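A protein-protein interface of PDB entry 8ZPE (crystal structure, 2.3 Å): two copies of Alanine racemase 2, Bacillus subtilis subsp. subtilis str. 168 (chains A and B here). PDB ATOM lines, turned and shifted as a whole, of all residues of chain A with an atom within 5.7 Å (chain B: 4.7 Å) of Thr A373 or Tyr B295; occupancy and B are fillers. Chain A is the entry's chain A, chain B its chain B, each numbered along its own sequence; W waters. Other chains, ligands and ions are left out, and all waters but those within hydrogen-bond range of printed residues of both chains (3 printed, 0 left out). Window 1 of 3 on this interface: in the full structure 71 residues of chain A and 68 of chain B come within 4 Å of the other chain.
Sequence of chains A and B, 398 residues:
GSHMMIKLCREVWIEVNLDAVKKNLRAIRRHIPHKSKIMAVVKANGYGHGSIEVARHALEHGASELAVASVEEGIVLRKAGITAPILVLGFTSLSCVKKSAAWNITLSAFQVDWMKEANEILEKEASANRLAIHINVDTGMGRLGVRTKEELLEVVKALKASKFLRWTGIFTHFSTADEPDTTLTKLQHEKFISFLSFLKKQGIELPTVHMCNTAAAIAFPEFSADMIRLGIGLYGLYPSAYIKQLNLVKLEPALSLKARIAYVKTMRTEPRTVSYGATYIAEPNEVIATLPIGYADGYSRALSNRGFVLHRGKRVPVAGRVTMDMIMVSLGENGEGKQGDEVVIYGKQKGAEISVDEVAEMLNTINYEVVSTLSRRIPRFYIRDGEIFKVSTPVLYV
Of the printed residues of chain B, Tyr A368 touches Tyr B295 and Met B324. Val A371 touches none of the printed residues of chain B. Thr A373 touches just one residue of chain B: Tyr B295 (3.3 Å). Tyr B295 touches just these residues of chain A: Ile A366 (3.98 Å), Tyr A368 (3.1 Å), Glu A369 (3.4 Å), Ser A372 (3.7 Å) and Thr A373 (3.3 Å). Of the printed residues of chain A, Ala B296 touches Ser A372. Printed residues of chain A within 4 Å of Ser B300: Glu A369 (3.7 Å). Of the printed residues of chain A, Arg B301 touches Ile A366 (3.4 Å) and Glu A369 (2.8 Å). Printed residues of chain A within 4 Å of Met B324: Tyr A368.
Among the printed residues, 10 pairs touch across the chains. Among the printed residues, no Asp or Glu carboxylate lies within 4 Å of a Lys or Arg side-chain nitrogen of the other chain.
Among the printed residues, merely in contact across the chains: Ile A366 with Tyr B295, Ile A366 with Arg B301, Tyr A368 with Tyr B295, Tyr A368 with Met B324, Glu A369 with Tyr B295, Glu A369 with Ser B300, Ser A372 with Tyr B295, Ser A372 with Ala B296 and Thr A373 with Tyr B295.
OE2 of Glu A369 is in hydrogen-bond range of N of Arg B301 (2.8 Å).
Positions printed for both chains: 297 and 298. Of the 10 pairs that touch across the chains among the printed residues, none has its exchanged pair printed and touching as well.
The side-chain hydroxyl (OG) of Ser A372 lies within hydrogen-bond range of the backbone carbonyl oxygen (O) of Tyr A368 (2.7 Å). O of Glu A369 sits at hydrogen-bond distance from OG1 of Thr A373 (2.7 Å). The backbone NH (N) of Tyr B295 sits at hydrogen-bond distance from the backbone carbonyl oxygen (O) of Thr B323 (3.1 Å). N of Tyr B295 sits at hydrogen-bond distance from O of Met B324 (3.2 Å). N of Ala B296 lies within hydrogen-bond range of O of Met B324 (3.2 Å).
Water W3 lies within hydrogen-bond range of OE1 of Glu A369 and OG of Ser B300. Water W2 bridges the backbone carbonyl oxygen of Tyr B295 (2.8 Å) and the side-chain carboxylate of Glu A369 (2.8 Å). Water W1 lies within hydrogen-bond range of the backbone carbonyl oxygen (O) of Ala B296 and the backbone carbonyl oxygen (O) of Ser A372.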
ATOM      1  N   GLY A  48      29.777 -27.021   8.634  1.00  0.00           N
ATOM      2  CA  GLY A  48      28.633 -27.524   9.369  1.00  0.00           C
ATOM      3  C   GLY A  48      28.836 -28.878  10.032  1.00  0.00           C
ATOM      4  O   GLY A  48      27.930 -29.348  10.747  1.00  0.00           O
ATOM      5  N   ASP A 297      16.632 -24.651  12.296  1.00  0.00           N
ATOM      6  CA  ASP A 297      17.728 -25.609  12.285  1.00  0.00           C
ATOM      7  C   ASP A 297      18.526 -25.593  10.983  1.00  0.00           C
ATOM      8  O   ASP A 297      19.583 -26.240  10.912  1.00  0.00           O
ATOM      9  CB  ASP A 297      17.196 -27.028  12.506  1.00  0.00           C
ATOM     10  CG  ASP A 297      16.463 -27.171  13.810  1.00  0.00           C
ATOM     11  OD1 ASP A 297      17.124 -27.104  14.858  1.00  0.00           O
ATOM     12  OD2 ASP A 297      15.227 -27.346  13.792  1.00  0.00           O
ATOM     13  N   GLY A 298      18.038 -24.897   9.955  1.00  0.00           N
ATOM     14  CA  GLY A 298      18.628 -24.931   8.637  1.00  0.00           C
ATOM     15  C   GLY A 298      17.890 -25.791   7.641  1.00  0.00           C
ATOM     16  O   GLY A 298      18.372 -25.953   6.516  1.00  0.00           O
ATOM     17  N   ILE A 366      23.862 -24.846  -3.712  1.00  0.00           N
ATOM     18  CA  ILE A 366      24.945 -25.810  -3.808  1.00  0.00           C
ATOM     19  C   ILE A 366      25.048 -26.534  -2.483  1.00  0.00           C
ATOM     20  O   ILE A 366      24.620 -26.026  -1.441  1.00  0.00           O
ATOM     21  CB  ILE A 366      26.281 -25.150  -4.172  1.00  0.00           C
ATOM     22  CG1 ILE A 366      26.467 -23.859  -3.355  1.00  0.00           C
ATOM     23  CG2 ILE A 366      26.302 -24.867  -5.682  1.00  0.00           C
ATOM     24  CD1 ILE A 366      27.895 -23.265  -3.393  1.00  0.00           C
ATOM     25  N   TYR A 368      27.461 -26.937  -0.550  1.00  0.00           N
ATOM     26  CA  TYR A 368      28.133 -26.098   0.447  1.00  0.00           C
ATOM     27  C   TYR A 368      27.154 -25.385   1.379  1.00  0.00           C
ATOM     28  O   TYR A 368      27.384 -25.300   2.586  1.00  0.00           O
ATOM     29  CB  TYR A 368      28.975 -25.022  -0.218  1.00  0.00           C
ATOM     30  CG  TYR A 368      30.168 -25.407  -1.072  1.00  0.00           C
ATOM     31  CD1 TYR A 368      30.003 -25.843  -2.387  1.00  0.00           C
ATOM     32  CD2 TYR A 368      31.462 -25.234  -0.596  1.00  0.00           C
ATOM     33  CE1 TYR A 368      31.105 -26.146  -3.197  1.00  0.00           C
ATOM     34  CE2 TYR A 368      32.569 -25.539  -1.387  1.00  0.00           C
ATOM     35  CZ  TYR A 368      32.378 -25.986  -2.686  1.00  0.00           C
ATOM     36  OH  TYR A 368      33.454 -26.273  -3.475  1.00  0.00           O
ATOM     37  N   GLU A 369      26.090 -24.808   0.831  1.00  0.00           N
ATOM     38  CA  GLU A 369      25.185 -24.023   1.663  1.00  0.00           C
ATOM     39  C   GLU A 369      24.283 -24.904   2.497  1.00  0.00           C
ATOM     40  O   GLU A 369      23.872 -24.514   3.594  1.00  0.00           O
ATOM     41  CB  GLU A 369      24.313 -23.094   0.812  1.00  0.00           C
ATOM     42  CG  GLU A 369      23.493 -22.169   1.659  1.00  0.00           C
ATOM     43  CD  GLU A 369      22.719 -21.139   0.874  1.00  0.00           C
ATOM     44  OE1 GLU A 369      22.221 -21.472  -0.227  1.00  0.00           O
ATOM     45  OE2 GLU A 369      22.576 -20.001   1.388  1.00  0.00           O
ATOM     46  N   VAL A 370      23.944 -26.081   1.985  1.00  0.00           N
ATOM     47  CA  VAL A 370      22.983 -26.916   2.681  1.00  0.00           C
ATOM     48  C   VAL A 370      23.566 -27.392   3.997  1.00  0.00           C
ATOM     49  O   VAL A 370      22.883 -27.364   5.028  1.00  0.00           O
ATOM     50  CB  VAL A 370      22.549 -28.080   1.775  1.00  0.00           C
ATOM     51  CG1 VAL A 370      21.916 -29.183   2.592  1.00  0.00           C
ATOM     52  CG2 VAL A 370      21.585 -27.550   0.713  1.00  0.00           C
ATOM     53  N   VAL A 371      24.856 -27.764   3.994  1.00  0.00           N
ATOM     54  CA  VAL A 371      25.522 -28.302   5.183  1.00  0.00           C
ATOM     55  C   VAL A 371      26.054 -27.202   6.109  1.00  0.00           C
ATOM     56  O   VAL A 371      26.055 -27.377   7.333  1.00  0.00           O
ATOM     57  CB  VAL A 371      26.657 -29.277   4.791  1.00  0.00           C
ATOM     58  CG1 VAL A 371      26.086 -30.537   4.201  1.00  0.00           C
ATOM     59  CG2 VAL A 371      27.655 -28.633   3.796  1.00  0.00           C
ATOM     60  N   SER A 372      26.526 -26.069   5.579  1.00  0.00           N
ATOM     61  CA  SER A 372      27.132 -25.126   6.509  1.00  0.00           C
ATOM     62  C   SER A 372      26.110 -24.219   7.170  1.00  0.00           C
ATOM     63  O   SER A 372      26.489 -23.432   8.048  1.00  0.00           O
ATOM     64  CB  SER A 372      28.189 -24.276   5.821  1.00  0.00           C
ATOM     65  OG  SER A 372      27.633 -23.641   4.690  1.00  0.00           O
ATOM     66  N   THR A 373      24.834 -24.305   6.787  1.00  0.00           N
ATOM     67  CA  THR A 373      23.792 -23.579   7.506  1.00  0.00           C
ATOM     68  C   THR A 373      23.052 -24.468   8.487  1.00  0.00           C
ATOM     69  O   THR A 373      21.991 -24.074   8.987  1.00  0.00           O
ATOM     70  CB  THR A 373      22.804 -22.940   6.537  1.00  0.00           C
ATOM     71  OG1 THR A 373      22.238 -23.955   5.708  1.00  0.00           O
ATOM     72  CG2 THR A 373      23.539 -21.951   5.665  1.00  0.00           C
ATOM     73  N   LEU A 374      23.579 -25.666   8.753  1.00  0.00           N
ATOM     74  CA  LEU A 374      22.996 -26.542   9.748  1.00  0.00           C
ATOM     75  C   LEU A 374      23.269 -25.963  11.129  1.00  0.00           C
ATOM     76  O   LEU A 374      24.427 -25.836  11.536  1.00  0.00           O
ATOM     77  CB  LEU A 374      23.556 -27.950   9.604  1.00  0.00           C
ATOM     78  CG  LEU A 374      22.905 -28.750   8.481  1.00  0.00           C
ATOM     79  CD1 LEU A 374      23.530 -30.110   8.374  1.00  0.00           C
ATOM     80  CD2 LEU A 374      21.416 -28.875   8.710  1.00  0.00           C
ATOM     81  N   SER A 375      22.195 -25.611  11.836  1.00  0.00           N
ATOM     82  CA  SER A 375      22.303 -24.864  13.083  1.00  0.00           C
ATOM     83  C   SER A 375      23.144 -25.601  14.123  1.00  0.00           C
ATOM     84  O   SER A 375      23.157 -26.830  14.203  1.00  0.00           O
ATOM     85  CB  SER A 375      20.908 -24.595  13.640  1.00  0.00           C
ATOM     86  OG  SER A 375      20.967 -24.042  14.946  1.00  0.00           O
ATOM     87  N   GLY B 294      28.764 -14.182   4.762  1.00  0.00           N
ATOM     88  CA  GLY B 294      28.512 -15.153   3.710  1.00  0.00           C
ATOM     89  C   GLY B 294      27.344 -16.075   4.010  1.00  0.00           C
ATOM     90  O   GLY B 294      26.640 -15.868   5.018  1.00  0.00           O
ATOM     91  N   TYR B 295      27.125 -17.098   3.164  1.00  0.00           N
ATOM     92  CA  TYR B 295      25.928 -17.914   3.345  1.00  0.00           C
ATOM     93  C   TYR B 295      25.990 -18.733   4.622  1.00  0.00           C
ATOM     94  O   TYR B 295      24.940 -19.008   5.216  1.00  0.00           O
ATOM     95  CB  TYR B 295      25.639 -18.812   2.132  1.00  0.00           C
ATOM     96  CG  TYR B 295      26.758 -19.664   1.563  1.00  0.00           C
ATOM     97  CD1 TYR B 295      27.139 -20.858   2.162  1.00  0.00           C
ATOM     98  CD2 TYR B 295      27.385 -19.301   0.366  1.00  0.00           C
ATOM     99  CE1 TYR B 295      28.138 -21.638   1.618  1.00  0.00           C
ATOM    100  CE2 TYR B 295      28.375 -20.071  -0.189  1.00  0.00           C
ATOM    101  CZ  TYR B 295      28.756 -21.238   0.445  1.00  0.00           C
ATOM    102  OH  TYR B 295      29.754 -22.003  -0.111  1.00  0.00           O
ATOM    103  N   ALA B 296      27.189 -19.077   5.103  1.00  0.00           N
ATOM    104  CA  ALA B 296      27.271 -19.819   6.360  1.00  0.00           C
ATOM    105  C   ALA B 296      26.862 -18.972   7.557  1.00  0.00           C
ATOM    106  O   ALA B 296      26.521 -19.528   8.603  1.00  0.00           O
ATOM    107  CB  ALA B 296      28.680 -20.383   6.576  1.00  0.00           C
ATOM    108  N   ASP B 297      26.848 -17.645   7.423  1.00  0.00           N
ATOM    109  CA  ASP B 297      26.325 -16.794   8.488  1.00  0.00           C
ATOM    110  C   ASP B 297      24.811 -16.676   8.453  1.00  0.00           C
ATOM    111  O   ASP B 297      24.227 -16.192   9.421  1.00  0.00           O
ATOM    112  CB  ASP B 297      26.951 -15.401   8.412  1.00  0.00           C
ATOM    113  CG  ASP B 297      28.448 -15.456   8.426  1.00  0.00           C
ATOM    114  OD1 ASP B 297      28.987 -15.875   9.476  1.00  0.00           O
ATOM    115  OD2 ASP B 297      29.091 -15.126   7.395  1.00  0.00           O
ATOM    116  N   GLY B 298      24.168 -17.118   7.376  1.00  0.00           N
ATOM    117  CA  GLY B 298      22.734 -16.995   7.225  1.00  0.00           C
ATOM    118  C   GLY B 298      22.328 -15.998   6.173  1.00  0.00           C
ATOM    119  O   GLY B 298      21.130 -15.717   6.035  1.00  0.00           O
ATOM    120  N   TYR B 299      23.290 -15.444   5.437  1.00  0.00           N
ATOM    121  CA  TYR B 299      23.018 -14.487   4.371  1.00  0.00           C
ATOM    122  C   TYR B 299      22.881 -15.314   3.095  1.00  0.00           C
ATOM    123  O   TYR B 299      23.869 -15.784   2.531  1.00  0.00           O
ATOM    124  CB  TYR B 299      24.120 -13.435   4.312  1.00  0.00           C
ATOM    125  CG  TYR B 299      23.782 -12.271   3.423  1.00  0.00           C
ATOM    126  CD1 TYR B 299      22.810 -11.341   3.789  1.00  0.00           C
ATOM    127  CD2 TYR B 299      24.412 -12.117   2.194  1.00  0.00           C
ATOM    128  CE1 TYR B 299      22.489 -10.289   2.945  1.00  0.00           C
ATOM    129  CE2 TYR B 299      24.099 -11.081   1.355  1.00  0.00           C
ATOM    130  CZ  TYR B 299      23.147 -10.171   1.727  1.00  0.00           C
ATOM    131  OH  TYR B 299      22.855  -9.146   0.856  1.00  0.00           O
ATOM    132  N   SER B 300      21.640 -15.541   2.677  1.00  0.00           N
ATOM    133  CA  SER B 300      21.339 -16.567   1.685  1.00  0.00           C
ATOM    134  C   SER B 300      22.202 -16.424   0.437  1.00  0.00           C
ATOM    135  O   SER B 300      22.444 -15.322  -0.056  1.00  0.00           O
ATOM    136  CB  SER B 300      19.858 -16.500   1.313  1.00  0.00           C
ATOM    137  OG  SER B 300      19.585 -17.331   0.209  1.00  0.00           O
ATOM    138  N   ARG B 301      22.695 -17.555  -0.055  1.00  0.00           N
ATOM    139  CA  ARG B 301      23.400 -17.545  -1.327  1.00  0.00           C
ATOM    140  C   ARG B 301      22.501 -17.047  -2.454  1.00  0.00           C
ATOM    141  O   ARG B 301      22.995 -16.536  -3.470  1.00  0.00           O
ATOM    142  CB  ARG B 301      23.914 -18.942  -1.643  1.00  0.00           C
ATOM    143  CG  ARG B 301      24.766 -19.013  -2.924  1.00  0.00           C
ATOM    144  CD  ARG B 301      25.385 -20.378  -3.043  1.00  0.00           C
ATOM    145  NE  ARG B 301      26.139 -20.532  -4.276  1.00  0.00           N
ATOM    146  CZ  ARG B 301      25.600 -20.837  -5.445  1.00  0.00           C
ATOM    147  NH1 ARG B 301      24.294 -20.999  -5.582  1.00  0.00           N
ATOM    148  NH2 ARG B 301      26.393 -20.992  -6.498  1.00  0.00           N
ATOM    149  N   VAL B 322      27.475 -14.907  -3.651  1.00  0.00           N
ATOM    150  CA  VAL B 322      27.774 -15.007  -2.234  1.00  0.00           C
ATOM    151  C   VAL B 322      28.667 -16.219  -2.011  1.00  0.00           C
ATOM    152  O   VAL B 322      28.424 -17.300  -2.565  1.00  0.00           O
ATOM    153  CB  VAL B 322      26.464 -15.100  -1.434  1.00  0.00           C
ATOM    154  CG1 VAL B 322      26.740 -15.356   0.037  1.00  0.00           C
ATOM    155  CG2 VAL B 322      25.670 -13.831  -1.615  1.00  0.00           C
ATOM    156  N   THR B 323      29.726 -16.038  -1.222  1.00  0.00           N
ATOM    157  CA  THR B 323      30.592 -17.149  -0.842  1.00  0.00           C
ATOM    158  C   THR B 323      30.380 -17.448   0.637  1.00  0.00           C
ATOM    159  O   THR B 323      29.580 -16.799   1.315  1.00  0.00           O
ATOM    160  CB  THR B 323      32.060 -16.858  -1.174  1.00  0.00           C
ATOM    161  OG1 THR B 323      32.619 -15.949  -0.215  1.00  0.00           O
ATOM    162  CG2 THR B 323      32.183 -16.267  -2.597  1.00  0.00           C
ATOM    163  N   MET B 324      31.079 -18.466   1.131  1.00  0.00           N
ATOM    164  CA  MET B 324      30.744 -18.993   2.448  1.00  0.00           C
ATOM    165  C   MET B 324      30.879 -17.929   3.530  1.00  0.00           C
ATOM    166  O   MET B 324      30.015 -17.814   4.412  1.00  0.00           O
ATOM    167  CB  MET B 324      31.619 -20.194   2.768  1.00  0.00           C
ATOM    168  CG  MET B 324      31.037 -21.057   3.853  1.00  0.00           C
ATOM    169  SD  MET B 324      31.956 -22.582   4.074  1.00  0.00           S
ATOM    170  CE  MET B 324      31.284 -23.578   2.737  1.00  0.00           C
HETATM  171  O   HOH W   1      24.421 -21.210   9.777  1.00  0.00           O
HETATM  172  O   HOH W   2      22.433 -19.091   4.068  1.00  0.00           O
HETATM  173  O   HOH W   3      20.410 -20.026  -1.560  1.00  0.00           O
